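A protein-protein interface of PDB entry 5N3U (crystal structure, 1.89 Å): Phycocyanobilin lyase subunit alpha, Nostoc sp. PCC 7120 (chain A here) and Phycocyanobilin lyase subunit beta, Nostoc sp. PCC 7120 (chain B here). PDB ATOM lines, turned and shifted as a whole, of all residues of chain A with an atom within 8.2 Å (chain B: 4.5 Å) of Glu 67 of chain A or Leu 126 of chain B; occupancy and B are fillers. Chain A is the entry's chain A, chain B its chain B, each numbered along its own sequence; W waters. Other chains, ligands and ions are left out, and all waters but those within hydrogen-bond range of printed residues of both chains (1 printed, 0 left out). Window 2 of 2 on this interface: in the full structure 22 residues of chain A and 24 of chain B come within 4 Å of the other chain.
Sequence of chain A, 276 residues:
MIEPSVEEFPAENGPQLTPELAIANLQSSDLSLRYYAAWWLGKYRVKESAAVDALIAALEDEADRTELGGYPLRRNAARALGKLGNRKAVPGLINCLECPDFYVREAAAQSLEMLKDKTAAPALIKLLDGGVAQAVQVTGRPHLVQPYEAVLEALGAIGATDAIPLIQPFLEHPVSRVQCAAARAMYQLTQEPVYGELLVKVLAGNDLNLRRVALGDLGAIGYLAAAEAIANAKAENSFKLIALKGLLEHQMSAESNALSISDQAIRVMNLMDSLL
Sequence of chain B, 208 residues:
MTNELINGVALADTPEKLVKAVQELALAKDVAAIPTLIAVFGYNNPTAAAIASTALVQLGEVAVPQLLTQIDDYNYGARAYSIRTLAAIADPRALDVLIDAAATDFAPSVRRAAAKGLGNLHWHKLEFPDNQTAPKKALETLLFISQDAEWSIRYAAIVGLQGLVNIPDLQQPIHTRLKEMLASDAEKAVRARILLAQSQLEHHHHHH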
ATOM      1  N   ASP A  64      32.399 -19.055  22.095  1.00  0.00           N
ATOM      2  CA  ASP A  64      31.414 -19.803  22.956  1.00  0.00           C
ATOM      3  C   ASP A  64      30.005 -19.274  22.709  1.00  0.00           C
ATOM      4  O   ASP A  64      29.716 -18.033  22.967  1.00  0.00           O
ATOM      5  CB  ASP A  64      31.812 -19.649  24.445  1.00  0.00           C
ATOM      6  CG  ASP A  64      31.101 -20.666  25.390  1.00  0.00           C
ATOM      7  OD1 ASP A  64      30.220 -21.392  24.892  1.00  0.00           O
ATOM      8  OD2 ASP A  64      31.470 -20.759  26.614  1.00  0.00           O
ATOM      9  N   ARG A  65      29.137 -20.161  22.223  1.00  0.00           N
ATOM     10  CA  ARG A  65      27.744 -19.858  21.990  1.00  0.00           C
ATOM     11  C   ARG A  65      26.871 -20.938  22.590  1.00  0.00           C
ATOM     12  O   ARG A  65      27.268 -22.103  22.598  1.00  0.00           O
ATOM     13  CB  ARG A  65      27.426 -19.754  20.521  1.00  0.00           C
ATOM     14  CG  ARG A  65      28.272 -18.780  19.729  1.00  0.00           C
ATOM     15  CD  ARG A  65      28.101 -17.309  20.221  1.00  0.00           C
ATOM     16  NE  ARG A  65      26.790 -16.751  20.000  1.00  0.00           N
ATOM     17  CZ  ARG A  65      26.402 -16.150  18.868  1.00  0.00           C
ATOM     18  NH1 ARG A  65      27.227 -16.065  17.799  1.00  0.00           N
ATOM     19  NH2 ARG A  65      25.190 -15.608  18.809  1.00  0.00           N
ATOM     20  N   THR A  66      25.660 -20.576  22.992  1.00  0.00           N
ATOM     21  CA  THR A  66      24.701 -21.524  23.543  1.00  0.00           C
ATOM     22  C   THR A  66      23.345 -21.344  22.875  1.00  0.00           C
ATOM     23  O   THR A  66      23.243 -20.682  21.858  1.00  0.00           O
ATOM     24  CB  THR A  66      24.661 -21.353  25.119  1.00  0.00           C
ATOM     25  OG1 THR A  66      23.951 -22.442  25.763  1.00  0.00           O
ATOM     26  CG2 THR A  66      23.934 -20.037  25.527  1.00  0.00           C
ATOM     27  N   GLU A  67      22.297 -21.908  23.479  1.00  0.00           N
ATOM     28  CA  GLU A  67      20.896 -21.758  23.101  1.00  0.00           C
ATOM     29  C   GLU A  67      20.513 -20.325  22.771  1.00  0.00           C
ATOM     30  O   GLU A  67      20.985 -19.394  23.427  1.00  0.00           O
ATOM     31  CB  GLU A  67      19.943 -22.219  24.226  1.00  0.00           C
ATOM     32  CG  GLU A  67      20.053 -23.673  24.604  1.00  0.00           C
ATOM     33  CD  GLU A  67      19.024 -24.167  25.675  1.00  0.00           C
ATOM     34  OE1 GLU A  67      18.107 -23.466  26.157  1.00  0.00           O
ATOM     35  OE2 GLU A  67      19.111 -25.350  26.033  1.00  0.00           O
ATOM     36  N   LEU A  68      19.733 -20.164  21.704  1.00  0.00           N
ATOM     37  CA  LEU A  68      19.162 -18.873  21.266  1.00  0.00           C
ATOM     38  C   LEU A  68      20.221 -17.850  21.021  1.00  0.00           C
ATOM     39  O   LEU A  68      20.022 -16.701  21.398  1.00  0.00           O
ATOM     40  CB  LEU A  68      18.225 -18.276  22.344  1.00  0.00           C
ATOM     41  CG  LEU A  68      17.110 -19.194  22.835  1.00  0.00           C
ATOM     42  CD1 LEU A  68      16.332 -18.477  23.936  1.00  0.00           C
ATOM     43  CD2 LEU A  68      16.186 -19.569  21.678  1.00  0.00           C
ATOM     44  N   GLY A  69      21.346 -18.267  20.468  1.00  0.00           N
ATOM     45  CA  GLY A  69      22.471 -17.396  20.211  1.00  0.00           C
ATOM     46  C   GLY A  69      23.135 -16.718  21.416  1.00  0.00           C
ATOM     47  O   GLY A  69      23.908 -15.749  21.259  1.00  0.00           O
ATOM     48  N   GLY A  70      22.949 -17.268  22.602  1.00  0.00           N
ATOM     49  CA  GLY A  70      23.699 -16.787  23.787  1.00  0.00           C
ATOM     50  C   GLY A  70      25.206 -16.811  23.722  1.00  0.00           C
ATOM     51  O   GLY A  70      25.815 -17.566  22.925  1.00  0.00           O
ATOM     52  N   TYR A  71      25.834 -15.993  24.577  1.00  0.00           N
ATOM     53  CA  TYR A  71      27.248 -15.864  24.623  1.00  0.00           C
ATOM     54  C   TYR A  71      27.715 -16.119  26.058  1.00  0.00           C
ATOM     55  O   TYR A  71      27.899 -15.166  26.819  1.00  0.00           O
ATOM     56  CB  TYR A  71      27.618 -14.436  24.246  1.00  0.00           C
ATOM     57  CG  TYR A  71      27.384 -14.024  22.799  1.00  0.00           C
ATOM     58  CD1 TYR A  71      26.190 -13.459  22.407  1.00  0.00           C
ATOM     59  CD2 TYR A  71      28.441 -14.073  21.854  1.00  0.00           C
ATOM     60  CE1 TYR A  71      26.007 -13.014  21.110  1.00  0.00           C
ATOM     61  CE2 TYR A  71      28.272 -13.678  20.558  1.00  0.00           C
ATOM     62  CZ  TYR A  71      27.066 -13.151  20.195  1.00  0.00           C
ATOM     63  OH  TYR A  71      26.852 -12.775  18.923  1.00  0.00           O
ATOM     64  N   PRO A  72      27.920 -17.395  26.457  1.00  0.00           N
ATOM     65  CA  PRO A  72      28.291 -17.689  27.862  1.00  0.00           C
ATOM     66  C   PRO A  72      29.508 -16.947  28.410  1.00  0.00           C
ATOM     67  O   PRO A  72      29.512 -16.511  29.528  1.00  0.00           O
ATOM     68  CB  PRO A  72      28.572 -19.196  27.850  1.00  0.00           C
ATOM     69  CG  PRO A  72      27.705 -19.708  26.753  1.00  0.00           C
ATOM     70  CD  PRO A  72      27.692 -18.630  25.682  1.00  0.00           C
ATOM     71  N   ARG A  75      28.680 -13.295  29.130  1.00  0.00           N
ATOM     72  CA  ARG A  75      27.914 -13.156  30.355  1.00  0.00           C
ATOM     73  C   ARG A  75      28.775 -13.181  31.598  1.00  0.00           C
ATOM     74  O   ARG A  75      28.690 -12.341  32.444  1.00  0.00           O
ATOM     75  CB  ARG A  75      26.867 -14.293  30.434  1.00  0.00           C
ATOM     76  CG  ARG A  75      25.880 -14.328  29.316  1.00  0.00           C
ATOM     77  CD  ARG A  75      25.107 -15.668  29.367  1.00  0.00           C
ATOM     78  NE  ARG A  75      24.132 -15.751  28.260  1.00  0.00           N
ATOM     79  CZ  ARG A  75      23.336 -16.799  28.055  1.00  0.00           C
ATOM     80  NH1 ARG A  75      23.408 -17.825  28.871  1.00  0.00           N
ATOM     81  NH2 ARG A  75      22.456 -16.829  27.045  1.00  0.00           N
ATOM     82  N   ASP A 101      21.907 -11.097  23.149  1.00  0.00           N
ATOM     83  CA  ASP A 101      21.648 -12.055  24.201  1.00  0.00           C
ATOM     84  C   ASP A 101      21.145 -11.296  25.463  1.00  0.00           C
ATOM     85  O   ASP A 101      21.879 -10.496  26.067  1.00  0.00           O
ATOM     86  CB  ASP A 101      22.963 -12.742  24.514  1.00  0.00           C
ATOM     87  CG  ASP A 101      22.881 -13.729  25.658  1.00  0.00           C
ATOM     88  OD1 ASP A 101      21.812 -13.914  26.290  1.00  0.00           O
ATOM     89  OD2 ASP A 101      23.949 -14.351  25.959  1.00  0.00           O
ATOM     90  N   TYR A 103      20.842 -12.172  28.464  1.00  0.00           N
ATOM     91  CA  TYR A 103      21.588 -12.424  29.680  1.00  0.00           C
ATOM     92  C   TYR A 103      22.921 -11.623  29.690  1.00  0.00           C
ATOM     93  O   TYR A 103      23.390 -11.260  30.737  1.00  0.00           O
ATOM     94  CB  TYR A 103      21.813 -13.905  29.913  1.00  0.00           C
ATOM     95  CG  TYR A 103      20.535 -14.587  30.239  1.00  0.00           C
ATOM     96  CD1 TYR A 103      19.956 -14.398  31.505  1.00  0.00           C
ATOM     97  CD2 TYR A 103      19.851 -15.334  29.288  1.00  0.00           C
ATOM     98  CE1 TYR A 103      18.674 -14.948  31.809  1.00  0.00           C
ATOM     99  CE2 TYR A 103      18.622 -15.926  29.586  1.00  0.00           C
ATOM    100  CZ  TYR A 103      18.051 -15.705  30.842  1.00  0.00           C
ATOM    101  OH  TYR A 103      16.831 -16.233  31.150  1.00  0.00           O
ATOM    102  N   ARG A 141       9.961 -17.622  27.098  1.00  0.00           N
ATOM    103  CA  ARG A 141      11.155 -17.034  27.687  1.00  0.00           C
ATOM    104  C   ARG A 141      10.947 -16.849  29.169  1.00  0.00           C
ATOM    105  O   ARG A 141       9.976 -16.284  29.587  1.00  0.00           O
ATOM    106  CB  ARG A 141      11.388 -15.634  27.103  1.00  0.00           C
ATOM    107  CG  ARG A 141      11.475 -15.540  25.627  1.00  0.00           C
ATOM    108  CD  ARG A 141      12.735 -16.224  25.135  1.00  0.00           C
ATOM    109  NE  ARG A 141      12.723 -15.975  23.712  1.00  0.00           N
ATOM    110  CZ  ARG A 141      12.731 -16.900  22.772  1.00  0.00           C
ATOM    111  NH1 ARG A 141      12.905 -18.160  23.076  1.00  0.00           N
ATOM    112  NH2 ARG A 141      12.670 -16.531  21.507  1.00  0.00           N
ATOM    113  N   PRO B  92      14.886 -28.615  28.285  1.00  0.00           N
ATOM    114  CA  PRO B  92      16.227 -28.149  27.899  1.00  0.00           C
ATOM    115  C   PRO B  92      16.437 -26.656  28.045  1.00  0.00           C
ATOM    116  O   PRO B  92      17.579 -26.197  27.960  1.00  0.00           O
ATOM    117  CB  PRO B  92      16.324 -28.619  26.408  1.00  0.00           C
ATOM    118  CG  PRO B  92      14.888 -28.600  25.961  1.00  0.00           C
ATOM    119  CD  PRO B  92      14.142 -29.121  27.103  1.00  0.00           C
ATOM    120  N   ARG B  93      15.398 -25.882  28.359  1.00  0.00           N
ATOM    121  CA  ARG B  93      15.608 -24.484  28.693  1.00  0.00           C
ATOM    122  C   ARG B  93      16.421 -24.299  29.989  1.00  0.00           C
ATOM    123  O   ARG B  93      16.953 -23.264  30.203  1.00  0.00           O
ATOM    124  CB  ARG B  93      14.326 -23.730  28.824  1.00  0.00           C
ATOM    125  CG  ARG B  93      13.532 -23.571  27.496  1.00  0.00           C
ATOM    126  CD  ARG B  93      12.243 -22.857  27.814  1.00  0.00           C
ATOM    127  NE  ARG B  93      11.315 -23.741  28.501  1.00  0.00           N
ATOM    128  CZ  ARG B  93      10.156 -23.351  29.034  1.00  0.00           C
ATOM    129  NH1 ARG B  93       9.736 -22.124  28.899  1.00  0.00           N
ATOM    130  NH2 ARG B  93       9.401 -24.223  29.682  1.00  0.00           N
ATOM    131  N   LEU B  95      19.248 -25.733  30.534  1.00  0.00           N
ATOM    132  CA  LEU B  95      20.669 -25.990  30.262  1.00  0.00           C
ATOM    133  C   LEU B  95      21.650 -24.996  30.975  1.00  0.00           C
ATOM    134  O   LEU B  95      22.592 -25.388  31.709  1.00  0.00           O
ATOM    135  CB  LEU B  95      20.883 -25.942  28.776  1.00  0.00           C
ATOM    136  CG  LEU B  95      22.335 -26.107  28.348  1.00  0.00           C
ATOM    137  CD1 LEU B  95      22.841 -27.499  28.602  1.00  0.00           C
ATOM    138  CD2 LEU B  95      22.598 -25.715  26.887  1.00  0.00           C
ATOM    139  N   TRP B 123      16.331 -32.621  24.535  1.00  0.00           N
ATOM    140  CA  TRP B 123      16.972 -31.761  23.580  1.00  0.00           C
ATOM    141  C   TRP B 123      16.160 -31.440  22.380  1.00  0.00           C
ATOM    142  O   TRP B 123      16.250 -30.308  21.875  1.00  0.00           O
ATOM    143  CB  TRP B 123      18.304 -32.333  23.137  1.00  0.00           C
ATOM    144  CG  TRP B 123      19.104 -32.864  24.203  1.00  0.00           C
ATOM    145  CD1 TRP B 123      19.463 -34.174  24.401  1.00  0.00           C
ATOM    146  CD2 TRP B 123      19.827 -32.099  25.190  1.00  0.00           C
ATOM    147  NE1 TRP B 123      20.309 -34.273  25.488  1.00  0.00           N
ATOM    148  CE2 TRP B 123      20.530 -33.021  26.004  1.00  0.00           C
ATOM    149  CE3 TRP B 123      19.878 -30.745  25.505  1.00  0.00           C
ATOM    150  CZ2 TRP B 123      21.272 -32.626  27.102  1.00  0.00           C
ATOM    151  CZ3 TRP B 123      20.634 -30.335  26.582  1.00  0.00           C
ATOM    152  CH2 TRP B 123      21.310 -31.280  27.391  1.00  0.00           C
ATOM    153  N   HIS B 124      15.278 -32.363  21.967  1.00  0.00           N
ATOM    154  CA  HIS B 124      14.503 -32.133  20.766  1.00  0.00           C
ATOM    155  C   HIS B 124      13.486 -31.076  20.978  1.00  0.00           C
ATOM    156  O   HIS B 124      12.924 -30.640  20.015  1.00  0.00           O
ATOM    157  CB  HIS B 124      13.733 -33.384  20.321  1.00  0.00           C
ATOM    158  CG  HIS B 124      12.626 -33.757  21.238  1.00  0.00           C
ATOM    159  ND1 HIS B 124      12.796 -34.654  22.279  1.00  0.00           N
ATOM    160  CD2 HIS B 124      11.333 -33.369  21.287  1.00  0.00           C
ATOM    161  CE1 HIS B 124      11.654 -34.828  22.908  1.00  0.00           C
ATOM    162  NE2 HIS B 124      10.760 -34.031  22.354  1.00  0.00           N
ATOM    163  N   LYS B 125      13.171 -30.694  22.229  1.00  0.00           N
ATOM    164  CA  LYS B 125      12.244 -29.607  22.442  1.00  0.00           C
ATOM    165  C   LYS B 125      12.737 -28.224  22.041  1.00  0.00           C
ATOM    166  O   LYS B 125      11.969 -27.270  22.053  1.00  0.00           O
ATOM    167  CB  LYS B 125      11.823 -29.637  23.882  1.00  0.00           C
ATOM    168  CG  LYS B 125      11.168 -30.992  24.278  1.00  0.00           C
ATOM    169  CD  LYS B 125       9.729 -30.905  24.720  1.00  0.00           C
ATOM    170  CE  LYS B 125       8.910 -30.114  23.698  1.00  0.00           C
ATOM    171  NZ  LYS B 125       7.522 -30.613  23.518  1.00  0.00           N
ATOM    172  N   LEU B 126      14.019 -28.110  21.754  1.00  0.00           N
ATOM    173  CA  LEU B 126      14.611 -26.878  21.324  1.00  0.00           C
ATOM    174  C   LEU B 126      14.517 -26.734  19.792  1.00  0.00           C
ATOM    175  O   LEU B 126      14.704 -27.685  19.061  1.00  0.00           O
ATOM    176  CB  LEU B 126      16.045 -26.839  21.664  1.00  0.00           C
ATOM    177  CG  LEU B 126      16.345 -26.829  23.166  1.00  0.00           C
ATOM    178  CD1 LEU B 126      17.846 -26.960  23.368  1.00  0.00           C
ATOM    179  CD2 LEU B 126      15.702 -25.644  23.866  1.00  0.00           C
ATOM    180  N   GLU B 127      14.324 -25.513  19.367  1.00  0.00           N
ATOM    181  CA  GLU B 127      14.223 -25.167  17.966  1.00  0.00           C
ATOM    182  C   GLU B 127      15.585 -25.360  17.302  1.00  0.00           C
ATOM    183  O   GLU B 127      16.636 -24.874  17.774  1.00  0.00           O
ATOM    184  CB  GLU B 127      13.677 -23.721  17.856  1.00  0.00           C
ATOM    185  CG  GLU B 127      13.557 -23.215  16.443  1.00  0.00           C
ATOM    186  CD  GLU B 127      12.726 -21.901  16.298  1.00  0.00           C
ATOM    187  OE1 GLU B 127      12.515 -21.173  17.300  1.00  0.00           O
ATOM    188  OE2 GLU B 127      12.274 -21.588  15.159  1.00  0.00           O
ATOM    189  N   PHE B 128      15.557 -26.023  16.163  1.00  0.00           N
ATOM    190  CA  PHE B 128      16.742 -26.368  15.391  1.00  0.00           C
ATOM    191  C   PHE B 128      17.521 -25.112  15.031  1.00  0.00           C
ATOM    192  O   PHE B 128      16.922 -24.087  14.657  1.00  0.00           O
ATOM    193  CB  PHE B 128      16.321 -27.120  14.147  1.00  0.00           C
ATOM    194  CG  PHE B 128      17.413 -27.496  13.267  1.00  0.00           C
ATOM    195  CD1 PHE B 128      17.977 -26.560  12.434  1.00  0.00           C
ATOM    196  CD2 PHE B 128      17.921 -28.791  13.280  1.00  0.00           C
ATOM    197  CE1 PHE B 128      19.088 -26.852  11.654  1.00  0.00           C
ATOM    198  CE2 PHE B 128      19.016 -29.117  12.469  1.00  0.00           C
ATOM    199  CZ  PHE B 128      19.587 -28.153  11.666  1.00  0.00           C
ATOM    200  N   ASP B 130      19.482 -25.538  17.862  1.00  0.00           N
ATOM    201  CA  ASP B 130      19.830 -25.575  19.344  1.00  0.00           C
ATOM    202  C   ASP B 130      19.673 -27.008  19.857  1.00  0.00           C
ATOM    203  O   ASP B 130      20.292 -27.384  20.822  1.00  0.00           O
ATOM    204  CB  ASP B 130      18.897 -24.616  20.089  1.00  0.00           C
ATOM    205  CG  ASP B 130      19.307 -23.205  19.916  1.00  0.00           C
ATOM    206  OD1 ASP B 130      20.423 -23.048  19.427  1.00  0.00           O
ATOM    207  OD2 ASP B 130      18.570 -22.239  20.293  1.00  0.00           O
ATOM    208  N   ASN B 131      18.803 -27.833  19.246  1.00  0.00           N
ATOM    209  CA  ASN B 131      18.706 -29.236  19.650  1.00  0.00           C
ATOM    210  C   ASN B 131      19.993 -30.037  19.436  1.00  0.00           C
ATOM    211  O   ASN B 131      20.223 -31.029  20.101  1.00  0.00           O
ATOM    212  CB  ASN B 131      17.532 -29.923  18.933  1.00  0.00           C
ATOM    213  CG  ASN B 131      17.776 -29.959  17.447  1.00  0.00           C
ATOM    214  OD1 ASN B 131      18.095 -28.935  16.848  1.00  0.00           O
ATOM    215  ND2 ASN B 131      17.731 -31.131  16.877  1.00  0.00           N
ATOM    216  N   ALA B 134      22.879 -27.660  22.097  1.00  0.00           N
ATOM    217  CA  ALA B 134      22.696 -27.787  23.510  1.00  0.00           C
ATOM    218  C   ALA B 134      23.400 -29.035  24.134  1.00  0.00           C
ATOM    219  O   ALA B 134      24.105 -28.911  25.167  1.00  0.00           O
ATOM    220  CB  ALA B 134      21.258 -27.801  23.812  1.00  0.00           C
HETATM  221  O   HOH W   1      19.543 -22.603  28.805  1.00  0.00           O
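The side-chain carboxylate (OE2) of Glu 67 of chain A lies close to the backbone carbonyl oxygen (O) of Pro 92 of chain B (2.6 Å). OD2 of Asp 130 of chain B sits at hydrogen-bond distance from N of Leu 68 of chain A (2.8 Å).
Among the printed residues, pairs that only touch across the chains: Thr 66 of chain A with Leu 95 of chain B (3.7 Å), Glu 67 of chain A with Arg 93 of chain B (3.7 Å), Glu 67 of chain A with Leu 95 of chain B (3.3 Å), Glu 67 of chain A with Leu 126 of chain B (3.4 Å), Glu 67 of chain A with Asp 130 of chain B (3.7 Å) and Glu 67 of chain A with Ala 134 of chain B (3.9 Å).
Glu 67 of chain A touches just these residues of chain B: Pro 92 (2.6 Å), Arg 93 (3.7 Å), Leu 95 (3.3 Å), Leu 126 (3.4 Å), Asp 130 (3.7 Å) and Ala 134 (3.9 Å). Of the printed residues of chain B, Leu 68 of chain A touches Asp 130 (2.8 Å). Printed residues of chain A within 4 Å of Leu 95 of chain B: Thr 66 and Glu 67. Of chain A, only Glu 67 comes within 4 Å of Leu 126 of chain B. Phe 128 of chain B touches none of the printed residues of chain A. Of the printed residues of chain A, Asp 130 of chain B touches Glu 67 and Leu 68. The nearest printed residue of chain B that does not touch Glu 67 of chain A is Trp 123 of chain B (5.2 Å). The nearest residue of chain A that does not touch Leu 126 of chain B is Leu 68 of chain A (6.5 Å).
Hydrophobic or aromatic side chains of chain B that line the printed part of chain A: Leu 95, Leu 126 and Ala 134. Among the printed residues, no Asp or Glu carboxylate lies within 4 Å of a Lys or Arg side-chain nitrogen of the other chain.
Water W1 lies within hydrogen-bond range of O of Arg 93 of chain B (3.0 Å) and OE1 of Glu 67 of chain A (3.1 Å).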
